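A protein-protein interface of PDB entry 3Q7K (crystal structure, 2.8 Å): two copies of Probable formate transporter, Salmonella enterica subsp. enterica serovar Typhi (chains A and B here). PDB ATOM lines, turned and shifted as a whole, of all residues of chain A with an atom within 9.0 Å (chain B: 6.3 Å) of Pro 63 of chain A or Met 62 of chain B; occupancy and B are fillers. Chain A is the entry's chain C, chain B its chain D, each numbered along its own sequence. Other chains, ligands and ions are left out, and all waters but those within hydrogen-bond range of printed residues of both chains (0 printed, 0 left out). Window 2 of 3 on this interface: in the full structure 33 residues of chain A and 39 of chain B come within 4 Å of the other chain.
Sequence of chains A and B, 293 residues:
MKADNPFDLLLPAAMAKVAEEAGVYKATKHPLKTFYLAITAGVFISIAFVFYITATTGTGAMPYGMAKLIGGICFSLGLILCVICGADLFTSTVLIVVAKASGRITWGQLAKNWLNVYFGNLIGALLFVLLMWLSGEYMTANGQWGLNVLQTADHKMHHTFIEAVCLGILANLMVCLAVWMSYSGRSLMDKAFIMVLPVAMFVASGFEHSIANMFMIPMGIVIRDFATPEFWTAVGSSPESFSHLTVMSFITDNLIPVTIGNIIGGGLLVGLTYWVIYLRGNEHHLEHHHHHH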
ATOM      1  N   THR A  56      20.365   5.120  16.937  1.00  0.00           N
ATOM      2  CA  THR A  56      21.007   4.047  16.220  1.00  0.00           C
ATOM      3  C   THR A  56      21.875   3.185  17.090  1.00  0.00           C
ATOM      4  O   THR A  56      22.499   2.279  16.600  1.00  0.00           O
ATOM      5  CB  THR A  56      21.827   4.547  15.026  1.00  0.00           C
ATOM      6  OG1 THR A  56      22.857   5.439  15.481  1.00  0.00           O
ATOM      7  CG2 THR A  56      20.911   5.208  13.992  1.00  0.00           C
ATOM      8  N   THR A  59      21.675  -0.963  16.857  1.00  0.00           N
ATOM      9  CA  THR A  59      20.923  -1.257  15.625  1.00  0.00           C
ATOM     10  C   THR A  59      21.647  -2.165  14.634  1.00  0.00           C
ATOM     11  O   THR A  59      21.108  -2.489  13.568  1.00  0.00           O
ATOM     12  CB  THR A  59      20.371   0.004  14.935  1.00  0.00           C
ATOM     13  OG1 THR A  59      21.424   0.933  14.671  1.00  0.00           O
ATOM     14  CG2 THR A  59      19.306   0.666  15.784  1.00  0.00           C
ATOM     15  N   GLY A  60      22.846  -2.606  15.028  1.00  0.00           N
ATOM     16  CA  GLY A  60      23.674  -3.601  14.295  1.00  0.00           C
ATOM     17  C   GLY A  60      22.974  -4.728  13.531  1.00  0.00           C
ATOM     18  O   GLY A  60      23.404  -5.080  12.441  1.00  0.00           O
ATOM     19  N   ALA A  61      21.906  -5.275  14.104  1.00  0.00           N
ATOM     20  CA  ALA A  61      21.153  -6.356  13.519  1.00  0.00           C
ATOM     21  C   ALA A  61      19.937  -5.929  12.666  1.00  0.00           C
ATOM     22  O   ALA A  61      19.355  -6.770  11.983  1.00  0.00           O
ATOM     23  CB  ALA A  61      20.711  -7.243  14.594  1.00  0.00           C
ATOM     24  N   MET A  62      19.525  -4.655  12.721  1.00  0.00           N
ATOM     25  CA  MET A  62      18.503  -4.122  11.828  1.00  0.00           C
ATOM     26  C   MET A  62      19.106  -4.003  10.427  1.00  0.00           C
ATOM     27  O   MET A  62      20.337  -3.805  10.297  1.00  0.00           O
ATOM     28  CB  MET A  62      18.125  -2.712  12.246  1.00  0.00           C
ATOM     29  CG  MET A  62      17.131  -2.586  13.352  1.00  0.00           C
ATOM     30  SD  MET A  62      16.770  -0.830  13.564  1.00  0.00           S
ATOM     31  CE  MET A  62      15.707  -0.511  12.135  1.00  0.00           C
ATOM     32  N   PRO A  63      18.255  -4.085   9.375  1.00  0.00           N
ATOM     33  CA  PRO A  63      18.710  -3.738   8.032  1.00  0.00           C
ATOM     34  C   PRO A  63      19.420  -2.393   8.035  1.00  0.00           C
ATOM     35  O   PRO A  63      18.890  -1.391   8.523  1.00  0.00           O
ATOM     36  CB  PRO A  63      17.414  -3.620   7.245  1.00  0.00           C
ATOM     37  CG  PRO A  63      16.434  -4.518   7.969  1.00  0.00           C
ATOM     38  CD  PRO A  63      16.821  -4.467   9.421  1.00  0.00           C
ATOM     39  N   TYR A  64      20.633  -2.391   7.515  1.00  0.00           N
ATOM     40  CA  TYR A  64      21.460  -1.214   7.348  1.00  0.00           C
ATOM     41  C   TYR A  64      20.692   0.059   7.036  1.00  0.00           C
ATOM     42  O   TYR A  64      20.669   0.999   7.830  1.00  0.00           O
ATOM     43  CB  TYR A  64      22.488  -1.474   6.244  1.00  0.00           C
ATOM     44  CG  TYR A  64      23.546  -0.426   6.153  1.00  0.00           C
ATOM     45  CD1 TYR A  64      24.733  -0.544   6.896  1.00  0.00           C
ATOM     46  CD2 TYR A  64      23.348   0.726   5.329  1.00  0.00           C
ATOM     47  CE1 TYR A  64      25.703   0.465   6.834  1.00  0.00           C
ATOM     48  CE2 TYR A  64      24.295   1.728   5.235  1.00  0.00           C
ATOM     49  CZ  TYR A  64      25.475   1.594   5.982  1.00  0.00           C
ATOM     50  OH  TYR A  64      26.427   2.588   5.887  1.00  0.00           O
ATOM     51  N   GLY A  65      20.080   0.093   5.864  1.00  0.00           N
ATOM     52  CA  GLY A  65      19.347   1.271   5.431  1.00  0.00           C
ATOM     53  C   GLY A  65      18.311   1.836   6.384  1.00  0.00           C
ATOM     54  O   GLY A  65      18.180   3.073   6.465  1.00  0.00           O
ATOM     55  N   MET A  66      17.577   0.942   7.077  1.00  0.00           N
ATOM     56  CA  MET A  66      16.484   1.325   7.970  1.00  0.00           C
ATOM     57  C   MET A  66      17.020   2.032   9.204  1.00  0.00           C
ATOM     58  O   MET A  66      16.527   3.078   9.648  1.00  0.00           O
ATOM     59  CB  MET A  66      15.633   0.114   8.349  1.00  0.00           C
ATOM     60  CG  MET A  66      14.865  -0.482   7.174  1.00  0.00           C
ATOM     61  SD  MET A  66      13.924   0.747   6.247  1.00  0.00           S
ATOM     62  CE  MET A  66      13.592  -0.116   4.692  1.00  0.00           C
ATOM     63  N   ALA A  67      18.077   1.475   9.736  1.00  0.00           N
ATOM     64  CA  ALA A  67      18.690   2.065  10.902  1.00  0.00           C
ATOM     65  C   ALA A  67      19.187   3.472  10.573  1.00  0.00           C
ATOM     66  O   ALA A  67      18.874   4.407  11.299  1.00  0.00           O
ATOM     67  CB  ALA A  67      19.816   1.167  11.441  1.00  0.00           C
ATOM     68  N   LYS A  68      19.935   3.616   9.473  1.00  0.00           N
ATOM     69  CA  LYS A  68      20.387   4.895   8.948  1.00  0.00           C
ATOM     70  C   LYS A  68      19.279   5.889   8.620  1.00  0.00           C
ATOM     71  O   LYS A  68      19.393   7.105   8.934  1.00  0.00           O
ATOM     72  CB  LYS A  68      21.159   4.647   7.663  1.00  0.00           C
ATOM     73  CG  LYS A  68      22.657   4.795   7.798  1.00  0.00           C
ATOM     74  CD  LYS A  68      23.239   3.987   8.961  1.00  0.00           C
ATOM     75  CE  LYS A  68      24.702   4.247   9.059  1.00  0.00           C
ATOM     76  NZ  LYS A  68      25.437   2.984   9.278  1.00  0.00           N
ATOM     77  N   LEU A  69      18.234   5.392   7.953  1.00  0.00           N
ATOM     78  CA  LEU A  69      17.105   6.237   7.635  1.00  0.00           C
ATOM     79  C   LEU A  69      16.468   6.840   8.894  1.00  0.00           C
ATOM     80  O   LEU A  69      16.171   8.041   8.897  1.00  0.00           O
ATOM     81  CB  LEU A  69      16.073   5.508   6.805  1.00  0.00           C
ATOM     82  CG  LEU A  69      14.716   6.192   6.760  1.00  0.00           C
ATOM     83  CD1 LEU A  69      14.744   7.452   5.889  1.00  0.00           C
ATOM     84  CD2 LEU A  69      13.728   5.184   6.235  1.00  0.00           C
ATOM     85  N   ILE A  70      16.295   6.025   9.948  1.00  0.00           N
ATOM     86  CA  ILE A  70      15.735   6.513  11.214  1.00  0.00           C
ATOM     87  C   ILE A  70      16.643   7.575  11.889  1.00  0.00           C
ATOM     88  O   ILE A  70      16.198   8.687  12.198  1.00  0.00           O
ATOM     89  CB  ILE A  70      15.230   5.341  12.153  1.00  0.00           C
ATOM     90  CG1 ILE A  70      13.880   4.806  11.645  1.00  0.00           C
ATOM     91  CG2 ILE A  70      14.983   5.818  13.556  1.00  0.00           C
ATOM     92  CD1 ILE A  70      13.743   3.333  11.799  1.00  0.00           C
ATOM     93  N   ALA B  55      18.050   3.752   1.867  1.00  0.00           N
ATOM     94  CA  ALA B  55      17.036   3.187   2.740  1.00  0.00           C
ATOM     95  C   ALA B  55      16.902   1.677   2.653  1.00  0.00           C
ATOM     96  O   ALA B  55      16.683   1.024   3.668  1.00  0.00           O
ATOM     97  CB  ALA B  55      15.684   3.848   2.475  1.00  0.00           C
ATOM     98  N   THR B  56      16.995   1.125   1.450  1.00  0.00           N
ATOM     99  CA  THR B  56      16.754  -0.310   1.260  1.00  0.00           C
ATOM    100  C   THR B  56      18.022  -1.166   1.289  1.00  0.00           C
ATOM    101  O   THR B  56      17.914  -2.381   1.169  1.00  0.00           O
ATOM    102  CB  THR B  56      16.019  -0.619  -0.035  1.00  0.00           C
ATOM    103  OG1 THR B  56      16.816  -0.128  -1.103  1.00  0.00           O
ATOM    104  CG2 THR B  56      14.637   0.048  -0.092  1.00  0.00           C
ATOM    105  N   THR B  57      19.198  -0.566   1.466  1.00  0.00           N
ATOM    106  CA  THR B  57      20.403  -1.366   1.496  1.00  0.00           C
ATOM    107  C   THR B  57      20.407  -2.279   2.718  1.00  0.00           C
ATOM    108  O   THR B  57      20.112  -1.851   3.844  1.00  0.00           O
ATOM    109  CB  THR B  57      21.655  -0.511   1.465  1.00  0.00           C
ATOM    110  OG1 THR B  57      21.769   0.111   0.176  1.00  0.00           O
ATOM    111  CG2 THR B  57      22.865  -1.380   1.726  1.00  0.00           C
ATOM    112  N   GLY B  58      20.716  -3.549   2.504  1.00  0.00           N
ATOM    113  CA  GLY B  58      20.666  -4.510   3.606  1.00  0.00           C
ATOM    114  C   GLY B  58      19.268  -4.990   3.979  1.00  0.00           C
ATOM    115  O   GLY B  58      19.093  -5.589   5.042  1.00  0.00           O
ATOM    116  N   THR B  59      18.267  -4.758   3.120  1.00  0.00           N
ATOM    117  CA  THR B  59      16.874  -5.095   3.494  1.00  0.00           C
ATOM    118  C   THR B  59      16.386  -6.424   2.920  1.00  0.00           C
ATOM    119  O   THR B  59      15.169  -6.722   2.954  1.00  0.00           O
ATOM    120  CB  THR B  59      15.849  -3.989   3.169  1.00  0.00           C
ATOM    121  OG1 THR B  59      15.719  -3.861   1.746  1.00  0.00           O
ATOM    122  CG2 THR B  59      16.225  -2.670   3.844  1.00  0.00           C
ATOM    123  N   GLY B  60      17.358  -7.211   2.437  1.00  0.00           N
ATOM    124  CA  GLY B  60      17.170  -8.565   1.919  1.00  0.00           C
ATOM    125  C   GLY B  60      16.290  -9.461   2.752  1.00  0.00           C
ATOM    126  O   GLY B  60      15.498 -10.222   2.193  1.00  0.00           O
ATOM    127  N   ALA B  61      16.402  -9.369   4.085  1.00  0.00           N
ATOM    128  CA  ALA B  61      15.618 -10.236   5.006  1.00  0.00           C
ATOM    129  C   ALA B  61      14.250  -9.679   5.404  1.00  0.00           C
ATOM    130  O   ALA B  61      13.446 -10.399   5.969  1.00  0.00           O
ATOM    131  CB  ALA B  61      16.436 -10.579   6.276  1.00  0.00           C
ATOM    132  N   MET B  62      14.005  -8.396   5.148  1.00  0.00           N
ATOM    133  CA  MET B  62      12.773  -7.742   5.559  1.00  0.00           C
ATOM    134  C   MET B  62      11.689  -8.226   4.656  1.00  0.00           C
ATOM    135  O   MET B  62      11.984  -8.628   3.555  1.00  0.00           O
ATOM    136  CB  MET B  62      12.902  -6.244   5.326  1.00  0.00           C
ATOM    137  CG  MET B  62      13.405  -5.450   6.478  1.00  0.00           C
ATOM    138  SD  MET B  62      13.236  -3.665   6.178  1.00  0.00           S
ATOM    139  CE  MET B  62      11.452  -3.491   6.365  1.00  0.00           C
ATOM    140  N   PRO B  63      10.417  -8.148   5.079  1.00  0.00           N
ATOM    141  CA  PRO B  63       9.357  -8.474   4.094  1.00  0.00           C
ATOM    142  C   PRO B  63       9.409  -7.543   2.879  1.00  0.00           C
ATOM    143  O   PRO B  63       9.542  -6.308   3.024  1.00  0.00           O
ATOM    144  CB  PRO B  63       8.048  -8.283   4.879  1.00  0.00           C
ATOM    145  CG  PRO B  63       8.453  -8.436   6.318  1.00  0.00           C
ATOM    146  CD  PRO B  63       9.844  -7.829   6.397  1.00  0.00           C
ATOM    147  N   TYR B  64       9.311  -8.169   1.706  1.00  0.00           N
ATOM    148  CA  TYR B  64       9.476  -7.521   0.408  1.00  0.00           C
ATOM    149  C   TYR B  64       8.779  -6.166   0.354  1.00  0.00           C
ATOM    150  O   TYR B  64       9.443  -5.111   0.222  1.00  0.00           O
ATOM    151  CB  TYR B  64       8.977  -8.446  -0.717  1.00  0.00           C
ATOM    152  CG  TYR B  64       9.195  -7.898  -2.097  1.00  0.00           C
ATOM    153  CD1 TYR B  64      10.374  -8.193  -2.817  1.00  0.00           C
ATOM    154  CD2 TYR B  64       8.250  -7.056  -2.674  1.00  0.00           C
ATOM    155  CE1 TYR B  64      10.591  -7.658  -4.095  1.00  0.00           C
ATOM    156  CE2 TYR B  64       8.451  -6.517  -3.922  1.00  0.00           C
ATOM    157  CZ  TYR B  64       9.605  -6.824  -4.648  1.00  0.00           C
ATOM    158  OH  TYR B  64       9.753  -6.246  -5.909  1.00  0.00           O
ATOM    159  N   GLY B  65       7.451  -6.208   0.463  1.00  0.00           N
ATOM    160  CA  GLY B  65       6.613  -5.008   0.387  1.00  0.00           C
ATOM    161  C   GLY B  65       6.985  -3.907   1.364  1.00  0.00           C
ATOM    162  O   GLY B  65       6.885  -2.732   1.011  1.00  0.00           O
ATOM    163  N   MET B  66       7.427  -4.270   2.578  1.00  0.00           N
ATOM    164  CA  MET B  66       7.740  -3.266   3.603  1.00  0.00           C
ATOM    165  C   MET B  66       9.002  -2.453   3.260  1.00  0.00           C
ATOM    166  O   MET B  66       8.976  -1.212   3.272  1.00  0.00           O
ATOM    167  CB  MET B  66       7.818  -3.891   4.989  1.00  0.00           C
ATOM    168  CG  MET B  66       6.471  -4.445   5.487  1.00  0.00           C
ATOM    169  SD  MET B  66       5.114  -3.210   5.647  1.00  0.00           S
ATOM    170  CE  MET B  66       3.651  -4.244   5.620  1.00  0.00           C
ATOM    171  N   ALA B  67      10.084  -3.149   2.930  1.00  0.00           N
ATOM    172  CA  ALA B  67      11.281  -2.536   2.385  1.00  0.00           C
ATOM    173  C   ALA B  67      10.993  -1.656   1.179  1.00  0.00           C
ATOM    174  O   ALA B  67      11.493  -0.535   1.099  1.00  0.00           O
ATOM    175  CB  ALA B  67      12.295  -3.581   2.034  1.00  0.00           C
ATOM    176  N   ILE B  70       9.046   1.573   2.196  1.00  0.00           N
ATOM    177  CA  ILE B  70       9.873   2.597   2.866  1.00  0.00           C
ATOM    178  C   ILE B  70      10.781   3.333   1.845  1.00  0.00           C
ATOM    179  O   ILE B  70      10.856   4.565   1.828  1.00  0.00           O
ATOM    180  CB  ILE B  70      10.652   2.042   4.065  1.00  0.00           C
ATOM    181  CG1 ILE B  70       9.691   1.779   5.250  1.00  0.00           C
ATOM    182  CG2 ILE B  70      11.698   3.050   4.510  1.00  0.00           C
ATOM    183  CD1 ILE B  70      10.189   0.766   6.313  1.00  0.00           C
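N of Gly 65 of chain A sits at hydrogen-bond distance from O of Thr 57 of chain B (2.8 Å). The side-chain sulfur (SD) of Met 66 of chain A lies close to the backbone carbonyl oxygen (O) of Ala 55 of chain B (3.8 Å).
The backbone carbonyl oxygen (O) of Thr 56 of chain B is in hydrogen-bond range of the side-chain hydroxyl (OG1) of Thr 59 of chain B (2.7 Å).
Among the printed residues, merely in contact across the chains: Pro 63 of chain A with Gly 58 of chain B, Pro 63 of chain A with Thr 59 of chain B, Pro 63 of chain A with Met 62 of chain B, Tyr 64 of chain A with Thr 57 of chain B, Gly 65 of chain A with Ala 55 of chain B, Met 66 of chain A with Thr 59 of chain B, Met 66 of chain A with Met 62 of chain B, Met 66 of chain A with Ile 70 of chain B and Leu 69 of chain A with Ile 70 of chain B.
Pro 63 of chain A touches just these residues of chain B: Gly 58, Thr 59 and Met 62. Of the printed residues of chain B, Met 66 of chain A touches Ala 55 (3.4 Å), Thr 59 (3.8 Å), Met 62 (3.7 Å) and Ile 70 (3.6 Å). Of the printed residues of chain A, Ala 55 of chain B touches Gly 65 and Met 66. Of the printed residues of chain A, Thr 57 of chain B touches Tyr 64 and Gly 65. No residue of chain A comes within 4 Å of Ala 61 of chain B. Met 62 of chain B touches just these residues of chain A: Pro 63 and Met 66. No residue of chain A comes within 4 Å of Pro 63 of chain B. The nearest residue of chain A that does not touch Met 62 of chain B is Met 62 of chain A (7.1 Å). The nearest printed residue of chain A that does not touch Gly 58 of chain B is Tyr 64 of chain A (4.3 Å).
Of the 13 printed residues of chain A, 5 touch a printed residue of chain B. Printed residues of chain A that touch a printed residue of chain B: Pro 63, Tyr 64, Gly 65, Met 66 and Leu 69. Hydrophobic or aromatic side chains of chain A that line the printed part of chain B: Pro 63, Tyr 64, Met 66 and Leu 69. Of the 14 printed residues of chain B, 6 touch a printed residue of chain A. Hydrophobic or aromatic side chains of chain B that line the printed part of chain A: Met 62 and Ile 70. Among the printed residues, no Asp or Glu carboxylate lies within 4 Å of a Lys or Arg side-chain nitrogen of the other chain.
Pro 63 of chain A touches Thr 59 of chain B, but with the chains exchanged Thr 59 of chain A does not touch Pro 63 of chain B (14.4 Å). Pro 63 of chain A touches Met 62 of chain B, but with the chains exchanged Met 62 of chain A does not touch Pro 63 of chain B (10.8 Å). Met 66 of chain A touches Thr 59 of chain B, but with the chains exchanged Thr 59 of chain A does not touch Met 66 of chain B (15.9 Å). Met 66 of chain A touches Ile 70 of chain B, but with the chains exchanged Ile 70 of chain A does not touch Met 66 of chain B (10.8 Å). 11 positions are printed for both chains.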
